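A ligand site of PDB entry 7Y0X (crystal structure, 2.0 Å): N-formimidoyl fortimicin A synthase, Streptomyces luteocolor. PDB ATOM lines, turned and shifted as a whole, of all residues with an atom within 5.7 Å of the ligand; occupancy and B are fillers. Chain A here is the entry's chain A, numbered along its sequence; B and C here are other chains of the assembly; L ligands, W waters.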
ATOM      1  N   ALA A 295      26.316  14.434   5.274  1.00  0.00           N
ATOM      2  CA  ALA A 295      26.427  15.810   5.793  1.00  0.00           C
ATOM      3  C   ALA A 295      25.485  15.995   6.982  1.00  0.00           C
ATOM      4  O   ALA A 295      24.252  15.734   6.848  1.00  0.00           O
ATOM      5  CB  ALA A 295      26.170  16.814   4.698  1.00  0.00           C
ATOM      6  N   PHE A 296      26.032  16.425   8.112  1.00  0.00           N
ATOM      7  CA  PHE A 296      25.274  16.794   9.341  1.00  0.00           C
ATOM      8  C   PHE A 296      24.396  15.614   9.772  1.00  0.00           C
ATOM      9  O   PHE A 296      23.226  15.832  10.137  1.00  0.00           O
ATOM     10  CB  PHE A 296      24.505  18.093   9.086  1.00  0.00           C
ATOM     11  CG  PHE A 296      25.408  19.254   8.735  1.00  0.00           C
ATOM     12  CD1 PHE A 296      26.460  19.607   9.567  1.00  0.00           C
ATOM     13  CD2 PHE A 296      25.216  19.985   7.575  1.00  0.00           C
ATOM     14  CE1 PHE A 296      27.283  20.684   9.255  1.00  0.00           C
ATOM     15  CE2 PHE A 296      26.045  21.056   7.268  1.00  0.00           C
ATOM     16  CZ  PHE A 296      27.081  21.395   8.105  1.00  0.00           C
ATOM     17  N   CYS A 298      22.848  13.232   8.354  1.00  0.00           N
ATOM     18  CA  CYS A 298      21.792  12.622   7.515  1.00  0.00           C
ATOM     19  C   CYS A 298      22.407  11.364   6.890  1.00  0.00           C
ATOM     20  O   CYS A 298      23.555  11.009   7.227  1.00  0.00           O
ATOM     21  CB  CYS A 298      21.264  13.600   6.476  1.00  0.00           C
ATOM     22  SG  CYS A 298      22.354  13.747   5.065  1.00  0.00           S
ATOM     23  N   ASN A 316      18.246  14.840   8.324  1.00  0.00           N
ATOM     24  CA  ASN A 316      18.549  15.241   9.713  1.00  0.00           C
ATOM     25  C   ASN A 316      18.890  16.720   9.700  1.00  0.00           C
ATOM     26  O   ASN A 316      19.714  17.115   8.881  1.00  0.00           O
ATOM     27  CB  ASN A 316      19.639  14.372  10.330  1.00  0.00           C
ATOM     28  CG  ASN A 316      19.853  14.683  11.798  1.00  0.00           C
ATOM     29  OD1 ASN A 316      18.914  14.914  12.539  1.00  0.00           O
ATOM     30  ND2 ASN A 316      21.109  14.724  12.206  1.00  0.00           N
ATOM     31  N   ALA A 317      18.240  17.476  10.553  1.00  0.00           N
ATOM     32  CA  ALA A 317      18.501  18.912  10.750  1.00  0.00           C
ATOM     33  C   ALA A 317      18.262  19.217  12.226  1.00  0.00           C
ATOM     34  O   ALA A 317      17.139  18.985  12.710  1.00  0.00           O
ATOM     35  CB  ALA A 317      17.603  19.762   9.863  1.00  0.00           C
ATOM     36  N   VAL A 318      19.306  19.683  12.910  1.00  0.00           N
ATOM     37  CA  VAL A 318      19.155  20.114  14.329  1.00  0.00           C
ATOM     38  C   VAL A 318      18.365  21.419  14.322  1.00  0.00           C
ATOM     39  O   VAL A 318      18.789  22.353  13.669  1.00  0.00           O
ATOM     40  CB  VAL A 318      20.514  20.255  15.035  1.00  0.00           C
ATOM     41  CG1 VAL A 318      20.306  20.809  16.444  1.00  0.00           C
ATOM     42  CG2 VAL A 318      21.232  18.914  15.084  1.00  0.00           C
ATOM     43  N   CYS A 319      17.246  21.451  15.040  1.00  0.00           N
ATOM     44  CA  CYS A 319      16.383  22.637  15.191  1.00  0.00           C
ATOM     45  C   CYS A 319      16.386  23.053  16.658  1.00  0.00           C
ATOM     46  O   CYS A 319      16.288  22.139  17.533  1.00  0.00           O
ATOM     47  CB  CYS A 319      14.981  22.349  14.670  1.00  0.00           C
ATOM     48  SG  CYS A 319      14.984  21.839  12.937  1.00  0.00           S
ATOM     49  N   ARG A 323       9.851  20.916  15.503  1.00  0.00           N
ATOM     50  CA  ARG A 323       9.105  21.011  14.228  1.00  0.00           C
ATOM     51  C   ARG A 323       8.534  19.643  13.939  1.00  0.00           C
ATOM     52  O   ARG A 323       9.287  18.650  14.037  1.00  0.00           O
ATOM     53  CB  ARG A 323      10.029  21.552  13.121  1.00  0.00           C
ATOM     54  CG  ARG A 323       9.489  21.391  11.715  1.00  0.00           C
ATOM     55  CD  ARG A 323      10.212  22.295  10.735  1.00  0.00           C
ATOM     56  NE  ARG A 323      11.624  21.994  10.559  1.00  0.00           N
ATOM     57  CZ  ARG A 323      12.112  21.023   9.791  1.00  0.00           C
ATOM     58  NH1 ARG A 323      11.299  20.209   9.144  1.00  0.00           N
ATOM     59  NH2 ARG A 323      13.416  20.876   9.659  1.00  0.00           N
ATOM     60  N   SER A 327       9.860  19.750   5.662  1.00  0.00           N
ATOM     61  CA  SER A 327      10.011  20.869   4.705  1.00  0.00           C
ATOM     62  C   SER A 327       9.981  20.275   3.283  1.00  0.00           C
ATOM     63  O   SER A 327      10.243  19.062   3.118  1.00  0.00           O
ATOM     64  CB  SER A 327      11.272  21.644   4.958  1.00  0.00           C
ATOM     65  OG  SER A 327      12.375  20.862   4.556  1.00  0.00           O
ATOM     66  N   ILE A 328       9.685  21.107   2.290  1.00  0.00           N
ATOM     67  CA  ILE A 328       9.748  20.706   0.855  1.00  0.00           C
ATOM     68  C   ILE A 328      11.148  20.174   0.564  1.00  0.00           C
ATOM     69  O   ILE A 328      11.253  19.113  -0.015  1.00  0.00           O
ATOM     70  CB  ILE A 328       9.386  21.886  -0.067  1.00  0.00           C
ATOM     71  CG1 ILE A 328       7.918  22.275   0.079  1.00  0.00           C
ATOM     72  CG2 ILE A 328       9.737  21.565  -1.503  1.00  0.00           C
ATOM     73  CD1 ILE A 328       6.983  21.128   0.042  1.00  0.00           C
ATOM     74  N   GLU A 329      12.181  20.925   0.973  1.00  0.00           N
ATOM     75  CA  GLU A 329      13.608  20.621   0.688  1.00  0.00           C
ATOM     76  C   GLU A 329      13.966  19.205   1.153  1.00  0.00           C
ATOM     77  O   GLU A 329      14.644  18.490   0.401  1.00  0.00           O
ATOM     78  CB  GLU A 329      14.456  21.668   1.410  1.00  0.00           C
ATOM     79  CG  GLU A 329      15.932  21.366   1.473  1.00  0.00           C
ATOM     80  CD  GLU A 329      16.691  22.398   2.280  1.00  0.00           C
ATOM     81  OE1 GLU A 329      17.681  22.925   1.740  1.00  0.00           O
ATOM     82  OE2 GLU A 329      16.280  22.701   3.435  1.00  0.00           O
ATOM     83  N   GLU A 330      13.550  18.847   2.375  1.00  0.00           N
ATOM     84  CA  GLU A 330      13.816  17.523   3.002  1.00  0.00           C
ATOM     85  C   GLU A 330      13.145  16.419   2.168  1.00  0.00           C
ATOM     86  O   GLU A 330      13.799  15.424   1.864  1.00  0.00           O
ATOM     87  CB  GLU A 330      13.315  17.496   4.444  1.00  0.00           C
ATOM     88  CG  GLU A 330      14.170  18.312   5.410  1.00  0.00           C
ATOM     89  CD  GLU A 330      13.513  18.725   6.737  1.00  0.00           C
ATOM     90  OE1 GLU A 330      12.261  18.643   6.865  1.00  0.00           O
ATOM     91  OE2 GLU A 330      14.273  19.094   7.675  1.00  0.00           O
ATOM     92  N   THR A 437      29.675  21.165   5.536  1.00  0.00           N
ATOM     93  CA  THR A 437      29.014  22.251   4.758  1.00  0.00           C
ATOM     94  C   THR A 437      29.249  21.960   3.264  1.00  0.00           C
ATOM     95  O   THR A 437      28.264  21.980   2.507  1.00  0.00           O
ATOM     96  CB  THR A 437      29.488  23.643   5.180  1.00  0.00           C
ATOM     97  OG1 THR A 437      29.263  23.786   6.582  1.00  0.00           O
ATOM     98  CG2 THR A 437      28.785  24.737   4.402  1.00  0.00           C
ATOM     99  N   THR A 440      27.165  19.118   1.786  1.00  0.00           N
ATOM    100  CA  THR A 440      25.763  19.424   1.389  1.00  0.00           C
ATOM    101  C   THR A 440      25.710  19.723  -0.118  1.00  0.00           C
ATOM    102  O   THR A 440      24.681  19.425  -0.738  1.00  0.00           O
ATOM    103  CB  THR A 440      25.082  20.557   2.177  1.00  0.00           C
ATOM    104  OG1 THR A 440      25.771  21.771   1.919  1.00  0.00           O
ATOM    105  CG2 THR A 440      25.033  20.290   3.668  1.00  0.00           C
ATOM    106  N   THR A 483      26.256  24.262  12.855  1.00  0.00           N
ATOM    107  CA  THR A 483      25.620  24.837  11.629  1.00  0.00           C
ATOM    108  C   THR A 483      24.261  25.437  12.019  1.00  0.00           C
ATOM    109  O   THR A 483      23.964  26.558  11.562  1.00  0.00           O
ATOM    110  CB  THR A 483      25.566  23.841  10.473  1.00  0.00           C
ATOM    111  OG1 THR A 483      25.174  24.618   9.347  1.00  0.00           O
ATOM    112  CG2 THR A 483      24.603  22.698  10.673  1.00  0.00           C
ATOM    113  N   ALA A 484      23.480  24.762  12.864  1.00  0.00           N
ATOM    114  CA  ALA A 484      22.177  25.280  13.324  1.00  0.00           C
ATOM    115  C   ALA A 484      22.390  26.626  14.045  1.00  0.00           C
ATOM    116  O   ALA A 484      21.636  27.569  13.788  1.00  0.00           O
ATOM    117  CB  ALA A 484      21.494  24.275  14.211  1.00  0.00           C
ATOM    118  N   PHE A 487      23.329  29.704  11.652  1.00  0.00           N
ATOM    119  CA  PHE A 487      22.212  30.260  10.833  1.00  0.00           C
ATOM    120  C   PHE A 487      20.989  30.554  11.700  1.00  0.00           C
ATOM    121  O   PHE A 487      19.922  30.719  11.149  1.00  0.00           O
ATOM    122  CB  PHE A 487      21.953  29.319   9.654  1.00  0.00           C
ATOM    123  CG  PHE A 487      23.146  29.252   8.727  1.00  0.00           C
ATOM    124  CD1 PHE A 487      23.469  30.333   7.920  1.00  0.00           C
ATOM    125  CD2 PHE A 487      23.997  28.164   8.744  1.00  0.00           C
ATOM    126  CE1 PHE A 487      24.597  30.310   7.111  1.00  0.00           C
ATOM    127  CE2 PHE A 487      25.130  28.128   7.934  1.00  0.00           C
ATOM    128  CZ  PHE A 487      25.424  29.206   7.121  1.00  0.00           C
ATOM    129  N   GLU B 451      19.574  27.137  -0.872  1.00  0.00           N
ATOM    130  CA  GLU B 451      20.111  27.947   0.262  1.00  0.00           C
ATOM    131  C   GLU B 451      21.559  28.389  -0.038  1.00  0.00           C
ATOM    132  O   GLU B 451      22.048  29.319   0.635  1.00  0.00           O
ATOM    133  CB  GLU B 451      20.032  27.191   1.590  1.00  0.00           C
ATOM    134  CG  GLU B 451      21.111  26.135   1.787  1.00  0.00           C
ATOM    135  CD  GLU B 451      20.834  24.757   1.196  1.00  0.00           C
ATOM    136  OE1 GLU B 451      19.849  24.652   0.400  1.00  0.00           O
ATOM    137  OE2 GLU B 451      21.619  23.785   1.498  1.00  0.00           O
ATOM    138  N   TRP B 452      22.250  27.776  -1.008  1.00  0.00           N
ATOM    139  CA  TRP B 452      23.712  28.025  -1.160  1.00  0.00           C
ATOM    140  C   TRP B 452      24.023  29.442  -1.659  1.00  0.00           C
ATOM    141  O   TRP B 452      24.955  30.076  -1.168  1.00  0.00           O
ATOM    142  CB  TRP B 452      24.371  26.965  -2.030  1.00  0.00           C
ATOM    143  CG  TRP B 452      25.090  25.921  -1.236  1.00  0.00           C
ATOM    144  CD1 TRP B 452      24.609  24.712  -0.823  1.00  0.00           C
ATOM    145  CD2 TRP B 452      26.421  26.019  -0.724  1.00  0.00           C
ATOM    146  NE1 TRP B 452      25.575  24.034  -0.126  1.00  0.00           N
ATOM    147  CE2 TRP B 452      26.693  24.808  -0.060  1.00  0.00           C
ATOM    148  CE3 TRP B 452      27.429  26.975  -0.821  1.00  0.00           C
ATOM    149  CZ2 TRP B 452      27.919  24.568   0.547  1.00  0.00           C
ATOM    150  CZ3 TRP B 452      28.641  26.738  -0.214  1.00  0.00           C
ATOM    151  CH2 TRP B 452      28.885  25.533   0.432  1.00  0.00           C
ATOM    152  N   MET B 455      23.890  31.948   1.161  1.00  0.00           N
ATOM    153  CA  MET B 455      25.035  31.631   2.050  1.00  0.00           C
ATOM    154  C   MET B 455      26.325  32.225   1.445  1.00  0.00           C
ATOM    155  O   MET B 455      27.089  32.887   2.191  1.00  0.00           O
ATOM    156  CB  MET B 455      25.168  30.116   2.226  1.00  0.00           C
ATOM    157  CG  MET B 455      26.094  29.705   3.336  1.00  0.00           C
ATOM    158  SD  MET B 455      25.831  27.995   3.861  1.00  0.00           S
ATOM    159  CE  MET B 455      26.500  27.093   2.470  1.00  0.00           C
ATOM    160  N   ASN C 347      11.045  26.298  -0.277  1.00  0.00           N
ATOM    161  CA  ASN C 347      11.987  25.202   0.013  1.00  0.00           C
ATOM    162  C   ASN C 347      11.998  24.911   1.521  1.00  0.00           C
ATOM    163  O   ASN C 347      11.975  23.725   1.903  1.00  0.00           O
ATOM    164  CB  ASN C 347      13.405  25.512  -0.500  1.00  0.00           C
ATOM    165  CG  ASN C 347      14.094  24.273  -1.006  1.00  0.00           C
ATOM    166  OD1 ASN C 347      13.447  23.349  -1.479  1.00  0.00           O
ATOM    167  ND2 ASN C 347      15.397  24.245  -0.903  1.00  0.00           N
ATOM    168  N   GLY C 348      11.993  25.969   2.333  1.00  0.00           N
ATOM    169  CA  GLY C 348      12.075  25.864   3.791  1.00  0.00           C
ATOM    170  C   GLY C 348      10.712  25.859   4.432  1.00  0.00           C
ATOM    171  O   GLY C 348      10.636  25.871   5.659  1.00  0.00           O
ATOM    172  N   SER C 349       9.648  25.794   3.621  1.00  0.00           N
ATOM    173  CA  SER C 349       8.267  25.882   4.123  1.00  0.00           C
ATOM    174  C   SER C 349       7.792  24.466   4.498  1.00  0.00           C
ATOM    175  O   SER C 349       8.330  23.499   3.951  1.00  0.00           O
ATOM    176  CB  SER C 349       7.393  26.583   3.110  1.00  0.00           C
ATOM    177  OG  SER C 349       7.797  27.965   2.963  1.00  0.00           O
HETATM  178  C1  LIG L   1      20.369  24.718   6.540  1.00  0.00           C
HETATM  179  C2  LIG L   1      24.331  24.469   4.284  1.00  0.00           C
HETATM  180  C3  LIG L   1      17.978  24.175   6.422  1.00  0.00           C
HETATM  181  C4  LIG L   1      15.870  23.383   6.824  1.00  0.00           C
HETATM  182  C5  LIG L   1      21.978  26.481   6.263  1.00  0.00           C
HETATM  183  C6  LIG L   1      14.444  23.276   6.391  1.00  0.00           C
HETATM  184  C7  LIG L   1      13.726  24.443   8.512  1.00  0.00           C
HETATM  185  C8  LIG L   1      15.220  24.527   8.881  1.00  0.00           C
HETATM  186  C9  LIG L   1      16.042  24.704   7.600  1.00  0.00           C
HETATM  187  C10 LIG L   1      22.159  27.729   5.460  1.00  0.00           C
HETATM  188  C11 LIG L   1      23.113  25.486   6.078  1.00  0.00           C
HETATM  189  N1  LIG L   1      20.632  19.032   7.202  1.00  0.00           N
HETATM  190  N2  LIG L   1      21.162  22.541   7.334  1.00  0.00           N
HETATM  191  C12 LIG L   1      21.452  23.674   6.472  1.00  0.00           C
HETATM  192  N3  LIG L   1      19.193  24.163   5.928  1.00  0.00           N
HETATM  193  C13 LIG L   1      21.072  20.208   7.967  1.00  0.00           C
HETATM  194  C14 LIG L   1      21.403  21.289   6.969  1.00  0.00           C
HETATM  195  O1  LIG L   1      21.853  21.005   5.862  1.00  0.00           O
HETATM  196  N4  LIG L   1      16.926  23.551   5.819  1.00  0.00           N
HETATM  197  O2  LIG L   1      14.168  22.760   5.306  1.00  0.00           O
HETATM  198  N5  LIG L   1      13.513  23.752   7.230  1.00  0.00           N
HETATM  199  O3  LIG L   1      15.592  23.353   9.636  1.00  0.00           O
HETATM  200  N6  LIG L   1      17.501  24.780   7.546  1.00  0.00           N
HETATM  201  O4  LIG L   1      20.739  25.898   5.839  1.00  0.00           O
HETATM  202  O5  LIG L   1      21.056  28.544   5.696  1.00  0.00           O
HETATM  203  O6  LIG L   1      23.203  25.114   4.681  1.00  0.00           O
HETATM  204  N7  LIG L   1      24.191  23.943   3.056  1.00  0.00           N
HETATM  205  O7  LIG L   1      25.329  24.361   4.971  1.00  0.00           O
HETATM  206  C15 LIG L   1      22.816  24.227   6.873  1.00  0.00           C
HETATM  207  O8  LIG L   1      22.813  24.526   8.261  1.00  0.00           O
HETATM  208  O   HOH W   1      26.868  24.941   7.282  1.00  0.00           O
HETATM  209  O   HOH W   2      12.761  24.208  11.824  1.00  0.00           O
HETATM  210  O   HOH W   3      19.431  22.804   3.743  1.00  0.00           O
HETATM  211  O   HOH W   4      22.443  17.678   5.307  1.00  0.00           O
HETATM  212  O   HOH W   5      10.624  23.806   7.668  1.00  0.00           O
HETATM  213  O   HOH W   6      19.439  28.366   7.680  1.00  0.00           O
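N7 of the ligand sits close to NE1 of Trp 452 of chain B, at 3.5 Å.
Merely in contact with the ligand: Thr 437 (3.5 Å), Phe 487 (3.6 Å), Met 455 of chain B (3.8 Å), Gly 348 of chain C (3.9 Å), Phe 296 (3.9 Å) and Ala 317 (3.98 Å).
Hydrophobic or aromatic side chains that line the ligand: Phe 296, Ala 317, Phe 487, Trp 452 of chain B and Met 455 of chain B.
Within 4 Å of the ligand: Phe 296, Asn 316, Ala 317, Cys 319, Arg 323, Ser 327, Glu 329, Thr 437, Thr 440, Thr 483, Phe 487, Glu 451 of chain B, Trp 452 of chain B, Met 455 of chain B and Gly 348 of chain C.
The nearest printed residue that does not touch the ligand is Asn 347 of chain C (4.2 Å).
The backbone NH of Ser 327 lies within hydrogen-bond range of the side-chain carboxylate of Glu 330 (2.9 Å).
N of Glu 329 lies within hydrogen-bond range of O of Asn 347 of chain C (3.0 Å).
The indole nitrogen (NE1) of Trp 452 of chain B is in hydrogen-bond range of the side-chain hydroxyl (OG1) of Thr 440 (3.1 Å).
The backbone carbonyl oxygen of Ala 317 sits at hydrogen-bond distance from the side-chain sulfur of Cys 319 (3.6 Å).
The side-chain carboxylate of Glu 330 is in salt-bridge range of the guanidinium group of Arg 323 (2.8 Å).
NH2 of Arg 323 is in hydrogen-bond range of SG of Cys 319.
ND2 of Asn 316 lies within hydrogen-bond range of O of Phe 296.
The side-chain hydroxyl (OG1) of Thr 440 is in hydrogen-bond range of the backbone carbonyl oxygen (O) of Thr 437 (2.6 Å).
Water W3 lies within hydrogen-bond range of OE1 of Glu 329, OE2 of Glu 451 of chain B and N4 of the ligand.
Water W1 lies within hydrogen-bond range of the side-chain hydroxyl (OG1) of Thr 483 (2.7 Å), the side-chain hydroxyl (OG1) of Thr 437 (2.7 Å) and an oxygen (O7) of the ligand (2.8 Å).
Water W5 bridges O of Gly 348 of chain C and N5 of the ligand.
Water W4 lies within hydrogen-bond range of N1 of the ligand and O of Ala 295.
Water W2 lies within hydrogen-bond range of the guanidinium group (NE) of Arg 323 and the side-chain sulfur (SG) of Cys 319.
An oxygen (O3) of the ligand sits at hydrogen-bond distance from the side-chain sulfur of Cys 319 (3.7 Å).
An oxygen (O8) of the ligand lies within hydrogen-bond range of the side-chain hydroxyl (OG1) of Thr 483, at 2.6 Å.
A nitrogen (N7) of the ligand lies within hydrogen-bond range of the side-chain carboxylate (OE2) of Glu 451 of chain B (3.0 Å).
An oxygen (O2) of the ligand is in hydrogen-bond range of the side-chain hydroxyl (OG) of Ser 327 (2.7 Å).
The backbone carbonyl oxygen of Asn 316 lies within hydrogen-bond range of a nitrogen (N1) of the ligand, at 2.7 Å.
NH2 of Arg 323 sits at hydrogen-bond distance from O3 of the ligand (3.3 Å).
OE2 of Glu 329 sits at hydrogen-bond distance from N4 of the ligand (2.6 Å).
The side-chain hydroxyl of Thr 440 sits at hydrogen-bond distance from a nitrogen (N7) of the ligand (2.9 Å).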
